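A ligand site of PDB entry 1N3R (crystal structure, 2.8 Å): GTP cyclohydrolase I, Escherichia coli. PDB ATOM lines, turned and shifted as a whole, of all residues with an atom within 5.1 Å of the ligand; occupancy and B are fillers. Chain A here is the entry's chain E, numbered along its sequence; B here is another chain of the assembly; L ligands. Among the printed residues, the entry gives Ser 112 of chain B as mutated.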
ATOM      1  N   THR A  87     -19.411  19.568   6.295  1.00  0.00           N
ATOM      2  CA  THR A  87     -19.576  20.360   7.502  1.00  0.00           C
ATOM      3  C   THR A  87     -20.864  19.920   8.165  1.00  0.00           C
ATOM      4  O   THR A  87     -21.915  19.880   7.529  1.00  0.00           O
ATOM      5  CB  THR A  87     -19.676  21.856   7.190  1.00  0.00           C
ATOM      6  OG1 THR A  87     -20.963  22.147   6.622  1.00  0.00           O
ATOM      7  CG2 THR A  87     -18.593  22.252   6.224  1.00  0.00           C
ATOM      8  N   TYR A 125     -31.575   9.653   6.664  1.00  0.00           N
ATOM      9  CA  TYR A 125     -30.714   9.163   7.723  1.00  0.00           C
ATOM     10  C   TYR A 125     -31.351   9.564   9.037  1.00  0.00           C
ATOM     11  O   TYR A 125     -32.376  10.247   9.046  1.00  0.00           O
ATOM     12  CB  TYR A 125     -29.308   9.744   7.598  1.00  0.00           C
ATOM     13  CG  TYR A 125     -29.197  11.232   7.901  1.00  0.00           C
ATOM     14  CD1 TYR A 125     -29.992  12.171   7.227  1.00  0.00           C
ATOM     15  CD2 TYR A 125     -28.289  11.697   8.856  1.00  0.00           C
ATOM     16  CE1 TYR A 125     -29.875  13.554   7.497  1.00  0.00           C
ATOM     17  CE2 TYR A 125     -28.159  13.069   9.143  1.00  0.00           C
ATOM     18  CZ  TYR A 125     -28.964  13.995   8.450  1.00  0.00           C
ATOM     19  OH  TYR A 125     -28.866  15.351   8.717  1.00  0.00           O
ATOM     20  N   VAL A 131     -25.674  16.570  12.683  1.00  0.00           N
ATOM     21  CA  VAL A 131     -26.599  16.821  11.576  1.00  0.00           C
ATOM     22  C   VAL A 131     -25.720  17.393  10.470  1.00  0.00           C
ATOM     23  O   VAL A 131     -24.848  18.221  10.735  1.00  0.00           O
ATOM     24  CB  VAL A 131     -27.668  17.856  11.932  1.00  0.00           C
ATOM     25  CG1 VAL A 131     -28.508  18.186  10.708  1.00  0.00           C
ATOM     26  CG2 VAL A 131     -28.535  17.314  13.054  1.00  0.00           C
ATOM     27  N   ILE A 132     -25.956  16.950   9.230  1.00  0.00           N
ATOM     28  CA  ILE A 132     -25.153  17.404   8.096  1.00  0.00           C
ATOM     29  C   ILE A 132     -25.872  18.529   7.350  1.00  0.00           C
ATOM     30  O   ILE A 132     -27.096  18.651   7.416  1.00  0.00           O
ATOM     31  CB  ILE A 132     -24.867  16.215   7.152  1.00  0.00           C
ATOM     32  CG1 ILE A 132     -23.752  16.592   6.164  1.00  0.00           C
ATOM     33  CG2 ILE A 132     -26.125  15.813   6.429  1.00  0.00           C
ATOM     34  CD1 ILE A 132     -23.274  15.444   5.306  1.00  0.00           C
ATOM     35  N   GLY A 133     -25.102  19.350   6.651  1.00  0.00           N
ATOM     36  CA  GLY A 133     -25.686  20.428   5.887  1.00  0.00           C
ATOM     37  C   GLY A 133     -26.429  19.751   4.771  1.00  0.00           C
ATOM     38  O   GLY A 133     -25.936  18.767   4.226  1.00  0.00           O
ATOM     39  N   LEU A 134     -27.605  20.235   4.428  1.00  0.00           N
ATOM     40  CA  LEU A 134     -28.392  19.614   3.376  1.00  0.00           C
ATOM     41  C   LEU A 134     -27.720  19.454   2.008  1.00  0.00           C
ATOM     42  O   LEU A 134     -27.754  18.370   1.420  1.00  0.00           O
ATOM     43  CB  LEU A 134     -29.701  20.380   3.219  1.00  0.00           C
ATOM     44  CG  LEU A 134     -30.672  20.298   4.395  1.00  0.00           C
ATOM     45  CD1 LEU A 134     -31.896  21.113   4.071  1.00  0.00           C
ATOM     46  CD2 LEU A 134     -31.029  18.846   4.660  1.00  0.00           C
ATOM     47  N   SER A 135     -27.108  20.511   1.517  1.00  0.00           N
ATOM     48  CA  SER A 135     -26.460  20.446   0.223  1.00  0.00           C
ATOM     49  C   SER A 135     -25.345  19.412   0.218  1.00  0.00           C
ATOM     50  O   SER A 135     -24.955  18.913  -0.826  1.00  0.00           O
ATOM     51  CB  SER A 135     -25.889  21.811  -0.148  1.00  0.00           C
ATOM     52  OG  SER A 135     -24.754  22.097   0.651  1.00  0.00           O
ATOM     53  N   LYS A 136     -24.840  19.069   1.397  1.00  0.00           N
ATOM     54  CA  LYS A 136     -23.759  18.098   1.482  1.00  0.00           C
ATOM     55  C   LYS A 136     -24.182  16.706   0.998  1.00  0.00           C
ATOM     56  O   LYS A 136     -23.389  15.976   0.390  1.00  0.00           O
ATOM     57  CB  LYS A 136     -23.260  18.010   2.933  1.00  0.00           C
ATOM     58  CG  LYS A 136     -22.829  19.330   3.537  1.00  0.00           C
ATOM     59  CD  LYS A 136     -21.920  20.105   2.618  1.00  0.00           C
ATOM     60  CE  LYS A 136     -21.425  21.363   3.301  1.00  0.00           C
ATOM     61  NZ  LYS A 136     -21.124  22.452   2.334  1.00  0.00           N
ATOM     62  N   ARG A 139     -24.357  16.764  -2.605  1.00  0.00           N
ATOM     63  CA  ARG A 139     -22.978  16.748  -3.093  1.00  0.00           C
ATOM     64  C   ARG A 139     -22.304  15.367  -3.026  1.00  0.00           C
ATOM     65  O   ARG A 139     -21.579  14.974  -3.940  1.00  0.00           O
ATOM     66  CB  ARG A 139     -22.109  17.749  -2.328  1.00  0.00           C
ATOM     67  CG  ARG A 139     -22.613  19.182  -2.337  1.00  0.00           C
ATOM     68  CD  ARG A 139     -21.464  20.172  -2.182  1.00  0.00           C
ATOM     69  NE  ARG A 139     -21.018  20.635  -3.485  1.00  0.00           N
ATOM     70  CZ  ARG A 139     -20.927  21.922  -3.821  1.00  0.00           C
ATOM     71  NH1 ARG A 139     -21.238  22.854  -2.934  1.00  0.00           N
ATOM     72  NH2 ARG A 139     -20.556  22.252  -5.047  1.00  0.00           N
ATOM     73  N   CYS B 110     -32.905  30.198   5.393  1.00  0.00           N
ATOM     74  CA  CYS B 110     -31.880  29.335   5.968  1.00  0.00           C
ATOM     75  C   CYS B 110     -30.819  30.181   6.716  1.00  0.00           C
ATOM     76  O   CYS B 110     -30.205  31.081   6.152  1.00  0.00           O
ATOM     77  CB  CYS B 110     -31.241  28.477   4.875  1.00  0.00           C
ATOM     78  SG  CYS B 110     -30.223  29.381   3.706  1.00  0.00           S
ATOM     79  N   SER B 112     -27.971  29.552   7.448  1.00  0.00           N
ATOM     80  CA  SER B 112     -26.634  29.350   6.929  1.00  0.00           C
ATOM     81  C   SER B 112     -26.293  30.306   5.800  1.00  0.00           C
ATOM     82  O   SER B 112     -25.122  30.596   5.570  1.00  0.00           O
ATOM     83  CB  SER B 112     -26.498  27.926   6.418  1.00  0.00           C
ATOM     84  OG  SER B 112     -27.424  27.714   5.360  1.00  0.00           O
ATOM     85  N   HIS B 113     -27.322  30.795   5.106  1.00  0.00           N
ATOM     86  CA  HIS B 113     -27.122  31.673   3.961  1.00  0.00           C
ATOM     87  C   HIS B 113     -28.035  32.873   3.813  1.00  0.00           C
ATOM     88  O   HIS B 113     -27.808  33.743   2.980  1.00  0.00           O
ATOM     89  CB  HIS B 113     -27.227  30.834   2.689  1.00  0.00           C
ATOM     90  CG  HIS B 113     -26.058  29.918   2.473  1.00  0.00           C
ATOM     91  ND1 HIS B 113     -24.929  30.310   1.788  1.00  0.00           N
ATOM     92  CD2 HIS B 113     -25.840  28.649   2.881  1.00  0.00           C
ATOM     93  CE1 HIS B 113     -24.058  29.320   1.799  1.00  0.00           C
ATOM     94  NE2 HIS B 113     -24.586  28.299   2.455  1.00  0.00           N
ATOM     95  N   ILE B 117     -36.452  29.773   1.960  1.00  0.00           N
ATOM     96  CA  ILE B 117     -36.813  28.368   2.182  1.00  0.00           C
ATOM     97  C   ILE B 117     -38.299  28.352   1.850  1.00  0.00           C
ATOM     98  O   ILE B 117     -39.099  28.966   2.556  1.00  0.00           O
ATOM     99  CB  ILE B 117     -36.635  27.905   3.655  1.00  0.00           C
ATOM    100  CG1 ILE B 117     -35.173  27.526   3.901  1.00  0.00           C
ATOM    101  CG2 ILE B 117     -37.473  26.686   3.950  1.00  0.00           C
ATOM    102  CD1 ILE B 117     -34.909  27.012   5.287  1.00  0.00           C
ATOM    103  N   GLN B 149     -33.665  29.972  10.001  1.00  0.00           N
ATOM    104  CA  GLN B 149     -33.887  28.598  10.453  1.00  0.00           C
ATOM    105  C   GLN B 149     -33.016  27.449   9.983  1.00  0.00           C
ATOM    106  O   GLN B 149     -32.146  27.568   9.123  1.00  0.00           O
ATOM    107  CB  GLN B 149     -35.347  28.210  10.172  1.00  0.00           C
ATOM    108  CG  GLN B 149     -36.357  28.795  11.126  1.00  0.00           C
ATOM    109  CD  GLN B 149     -36.373  28.086  12.471  1.00  0.00           C
ATOM    110  OE1 GLN B 149     -35.374  27.467  12.870  1.00  0.00           O
ATOM    111  NE2 GLN B 149     -37.492  28.183  13.178  1.00  0.00           N
ATOM    112  N   VAL B 150     -33.273  26.323  10.623  1.00  0.00           N
ATOM    113  CA  VAL B 150     -32.653  25.057  10.322  1.00  0.00           C
ATOM    114  C   VAL B 150     -33.941  24.259  10.250  1.00  0.00           C
ATOM    115  O   VAL B 150     -34.667  24.221  11.230  1.00  0.00           O
ATOM    116  CB  VAL B 150     -31.808  24.541  11.481  1.00  0.00           C
ATOM    117  CG1 VAL B 150     -31.457  23.078  11.262  1.00  0.00           C
ATOM    118  CG2 VAL B 150     -30.567  25.386  11.602  1.00  0.00           C
ATOM    119  N   GLN B 151     -34.234  23.652   9.094  1.00  0.00           N
ATOM    120  CA  GLN B 151     -35.499  22.912   8.951  1.00  0.00           C
ATOM    121  C   GLN B 151     -35.681  21.879  10.047  1.00  0.00           C
ATOM    122  O   GLN B 151     -36.777  21.698  10.550  1.00  0.00           O
ATOM    123  CB  GLN B 151     -35.619  22.248   7.568  1.00  0.00           C
ATOM    124  CG  GLN B 151     -37.072  21.911   7.201  1.00  0.00           C
ATOM    125  CD  GLN B 151     -37.218  21.099   5.922  1.00  0.00           C
ATOM    126  OE1 GLN B 151     -36.731  21.495   4.854  1.00  0.00           O
ATOM    127  NE2 GLN B 151     -37.906  19.963   6.009  1.00  0.00           N
ATOM    128  N   GLU B 152     -34.597  21.221  10.413  1.00  0.00           N
ATOM    129  CA  GLU B 152     -34.664  20.226  11.459  1.00  0.00           C
ATOM    130  C   GLU B 152     -35.184  20.884  12.737  1.00  0.00           C
ATOM    131  O   GLU B 152     -36.199  20.472  13.296  1.00  0.00           O
ATOM    132  CB  GLU B 152     -33.279  19.618  11.675  1.00  0.00           C
ATOM    133  CG  GLU B 152     -32.791  18.730  10.536  1.00  0.00           C
ATOM    134  CD  GLU B 152     -31.966  19.461   9.470  1.00  0.00           C
ATOM    135  OE1 GLU B 152     -32.205  20.668   9.245  1.00  0.00           O
ATOM    136  OE2 GLU B 152     -31.085  18.812   8.847  1.00  0.00           O
ATOM    137  N   HIS B 179     -34.836  24.440  -0.412  1.00  0.00           N
ATOM    138  CA  HIS B 179     -33.868  25.404   0.083  1.00  0.00           C
ATOM    139  C   HIS B 179     -33.153  25.990  -1.115  1.00  0.00           C
ATOM    140  O   HIS B 179     -32.487  25.257  -1.858  1.00  0.00           O
ATOM    141  CB  HIS B 179     -32.867  24.709   1.008  1.00  0.00           C
ATOM    142  CG  HIS B 179     -33.465  24.235   2.308  1.00  0.00           C
ATOM    143  ND1 HIS B 179     -32.826  24.396   3.514  1.00  0.00           N
ATOM    144  CD2 HIS B 179     -34.628  23.608   2.574  1.00  0.00           C
ATOM    145  CE1 HIS B 179     -33.574  23.883   4.479  1.00  0.00           C
ATOM    146  NE2 HIS B 179     -34.676  23.399   3.936  1.00  0.00           N
ATOM    147  N   CYS B 181     -30.648  27.624  -1.097  1.00  0.00           N
ATOM    148  CA  CYS B 181     -29.215  27.648  -0.806  1.00  0.00           C
ATOM    149  C   CYS B 181     -28.657  26.301  -1.285  1.00  0.00           C
ATOM    150  O   CYS B 181     -27.449  26.008  -1.192  1.00  0.00           O
ATOM    151  CB  CYS B 181     -28.965  27.856   0.705  1.00  0.00           C
ATOM    152  SG  CYS B 181     -29.531  26.575   1.881  1.00  0.00           S
ATOM    153  N   VAL B 182     -29.579  25.486  -1.803  1.00  0.00           N
ATOM    154  CA  VAL B 182     -29.289  24.173  -2.360  1.00  0.00           C
ATOM    155  C   VAL B 182     -29.619  24.261  -3.837  1.00  0.00           C
ATOM    156  O   VAL B 182     -28.866  23.778  -4.698  1.00  0.00           O
ATOM    157  CB  VAL B 182     -30.192  23.077  -1.771  1.00  0.00           C
ATOM    158  CG1 VAL B 182     -29.862  21.743  -2.409  1.00  0.00           C
ATOM    159  CG2 VAL B 182     -30.061  23.026  -0.249  1.00  0.00           C
ATOM    160  N   ARG B 185     -27.919  28.030  -5.817  1.00  0.00           N
ATOM    161  CA  ARG B 185     -26.506  28.295  -5.714  1.00  0.00           C
ATOM    162  C   ARG B 185     -25.729  27.119  -5.121  1.00  0.00           C
ATOM    163  O   ARG B 185     -26.302  26.244  -4.465  1.00  0.00           O
ATOM    164  CB  ARG B 185     -26.318  29.588  -4.916  1.00  0.00           C
ATOM    165  CG  ARG B 185     -25.282  29.538  -3.829  1.00  0.00           C
ATOM    166  CD  ARG B 185     -25.916  29.542  -2.455  1.00  0.00           C
ATOM    167  NE  ARG B 185     -25.410  28.468  -1.609  1.00  0.00           N
ATOM    168  CZ  ARG B 185     -24.128  28.133  -1.506  1.00  0.00           C
ATOM    169  NH1 ARG B 185     -23.215  28.785  -2.196  1.00  0.00           N
ATOM    170  NH2 ARG B 185     -23.742  27.150  -0.700  1.00  0.00           N
ATOM    171  N   GLY B 186     -24.416  27.080  -5.359  1.00  0.00           N
ATOM    172  CA  GLY B 186     -23.612  25.996  -4.841  1.00  0.00           C
ATOM    173  C   GLY B 186     -23.747  24.783  -5.734  1.00  0.00           C
ATOM    174  O   GLY B 186     -23.388  24.843  -6.921  1.00  0.00           O
ATOM    175  N   ILE B 187     -24.275  23.687  -5.197  1.00  0.00           N
ATOM    176  CA  ILE B 187     -24.451  22.455  -5.963  1.00  0.00           C
ATOM    177  C   ILE B 187     -25.528  22.667  -7.020  1.00  0.00           C
ATOM    178  O   ILE B 187     -25.554  21.976  -8.033  1.00  0.00           O
ATOM    179  CB  ILE B 187     -24.837  21.258  -5.053  1.00  0.00           C
ATOM    180  CG1 ILE B 187     -24.605  19.951  -5.787  1.00  0.00           C
ATOM    181  CG2 ILE B 187     -26.293  21.337  -4.642  1.00  0.00           C
ATOM    182  CD1 ILE B 187     -23.166  19.701  -6.220  1.00  0.00           C
HETATM  183  P1  LIG L   1     -22.275  24.618  -0.139  1.00  0.00           P
HETATM  184  O1  LIG L   1     -21.660  25.635  -1.093  1.00  0.00           O
HETATM  185  O2  LIG L   1     -21.494  23.325   0.030  1.00  0.00           O
HETATM  186  O3  LIG L   1     -23.656  24.406  -0.520  1.00  0.00           O
HETATM  187  O4  LIG L   1     -22.294  25.426   1.311  1.00  0.00           O
HETATM  188  P2  LIG L   1     -21.108  26.277   2.082  1.00  0.00           P
HETATM  189  O5  LIG L   1     -19.949  26.450   1.098  1.00  0.00           O
HETATM  190  O6  LIG L   1     -21.684  27.534   2.570  1.00  0.00           O
HETATM  191  O7  LIG L   1     -20.708  25.323   3.243  1.00  0.00           O
HETATM  192  P3  LIG L   1     -20.814  25.486   4.839  1.00  0.00           P
HETATM  193  O8  LIG L   1     -19.819  24.672   5.486  1.00  0.00           O
HETATM  194  O9  LIG L   1     -20.747  26.987   5.105  1.00  0.00           O
HETATM  195  O10 LIG L   1     -22.280  24.803   5.240  1.00  0.00           O
HETATM  196  C1  LIG L   1     -23.490  25.498   4.693  1.00  0.00           C
HETATM  197  C2  LIG L   1     -24.427  24.197   4.732  1.00  0.00           C
HETATM  198  O11 LIG L   1     -25.662  24.201   5.562  1.00  0.00           O
HETATM  199  C3  LIG L   1     -24.869  23.638   3.445  1.00  0.00           C
HETATM  200  O12 LIG L   1     -24.611  22.265   3.332  1.00  0.00           O
HETATM  201  C4  LIG L   1     -26.375  24.018   3.257  1.00  0.00           C
HETATM  202  O13 LIG L   1     -26.989  23.316   2.329  1.00  0.00           O
HETATM  203  C5  LIG L   1     -26.728  23.585   4.824  1.00  0.00           C
HETATM  204  N1  LIG L   1     -28.133  24.032   5.259  1.00  0.00           N
HETATM  205  C6  LIG L   1     -28.789  25.199   4.839  1.00  0.00           C
HETATM  206  N2  LIG L   1     -29.955  25.016   5.523  1.00  0.00           N
HETATM  207  C7  LIG L   1     -30.039  23.858   6.302  1.00  0.00           C
HETATM  208  C8  LIG L   1     -31.000  23.405   7.042  1.00  0.00           C
HETATM  209  O14 LIG L   1     -32.171  23.715   7.411  1.00  0.00           O
HETATM  210  N3  LIG L   1     -30.616  22.075   7.709  1.00  0.00           N
HETATM  211  C9  LIG L   1     -29.435  21.613   7.429  1.00  0.00           C
HETATM  212  N4  LIG L   1     -29.077  20.308   8.087  1.00  0.00           N
HETATM  213  N5  LIG L   1     -28.433  22.078   6.649  1.00  0.00           N
HETATM  214  C10 LIG L   1     -28.861  23.260   6.108  1.00  0.00           C
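An oxygen (O2) of the ligand lies within salt-bridge range of the side-chain amino group of Lys 136 (2.5 Å).
NH1 of Arg 139 lies within salt-bridge range of O2 of the ligand (3.0 Å).
An oxygen (O13) of the ligand sits at hydrogen-bond distance from the backbone NH (N) of Ser 135 (2.9 Å).
The side-chain carboxylate of Glu 152 of chain B lies within hydrogen-bond range of a nitrogen (N4) of the ligand (2.6 Å).
O14 of the ligand is in hydrogen-bond range of N of Gln 151 of chain B.
An oxygen (O8) of the ligand sits close to the side-chain hydroxyl (OG1) of Thr 87, 3.0 Å away.
N5 of the ligand lies within hydrogen-bond range of N of Leu 134 (3.0 Å).
The backbone carbonyl oxygen (O) of Ile 132 sits at hydrogen-bond distance from a nitrogen (N4) of the ligand (2.7 Å).
O12 of the ligand lies within hydrogen-bond range of OG of Ser 135, at 2.7 Å.
The guanidinium group (NH2) of Arg 185 of chain B is in salt-bridge range of an oxygen (O1) of the ligand (2.6 Å).
A ring nitrogen (NE2) of His 113 of chain B sits at hydrogen-bond distance from an oxygen (O6) of the ligand.
The backbone NH (N) of Ile 132 is in hydrogen-bond range of the side-chain hydroxyl (OH) of Tyr 125, at 3.4 Å.
The backbone NH (N) of His 113 of chain B sits close to the side-chain sulfur (SG) of Cys 110 of chain B, at 3.5 Å.
The side-chain hydroxyl (OG) of Ser 112 of chain B is in hydrogen-bond range of the side-chain sulfur (SG) of Cys 110 of chain B (3.7 Å).
A ring nitrogen (NE2) of His 113 of chain B sits close to the guanidinium group (NH2) of Arg 185 of chain B (3.5 Å).
The side-chain amide oxygen of Gln 151 of chain B sits at hydrogen-bond distance from a ring nitrogen (NE2) of His 179 of chain B.
The guanidinium group (NE) of Arg 185 of chain B lies within hydrogen-bond range of the backbone carbonyl oxygen (O) of Cys 181 of chain B (3.2 Å).
O of Thr 87 is in hydrogen-bond range of N of Gly 133, at 3.3 Å.
SG of Cys 181 of chain B is in hydrogen-bond range of SG of Cys 110 of chain B (3.4 Å).
Merely in contact with the ligand: Val 131 (3.4 Å), Gly 133 (3.3 Å), Cys 110 of chain B (3.7 Å), Ser 112 of chain B (2.9 Å), Val 150 of chain B (3.2 Å), His 179 of chain B (3.3 Å) and Cys 181 of chain B (3.3 Å).
Hydrophobic or aromatic side chains that line the ligand: Val 131, Leu 134, His 113 of chain B, Val 150 of chain B and His 179 of chain B.
Within 4 Å of the ligand: Thr 87, Val 131, Ile 132, Gly 133, Leu 134, Ser 135, Lys 136, Arg 139, Cys 110 of chain B, Ser 112 of chain B, His 113 of chain B, Val 150 of chain B, Gln 151 of chain B, Glu 152 of chain B, His 179 of chain B, Cys 181 of chain B and Arg 185 of chain B.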
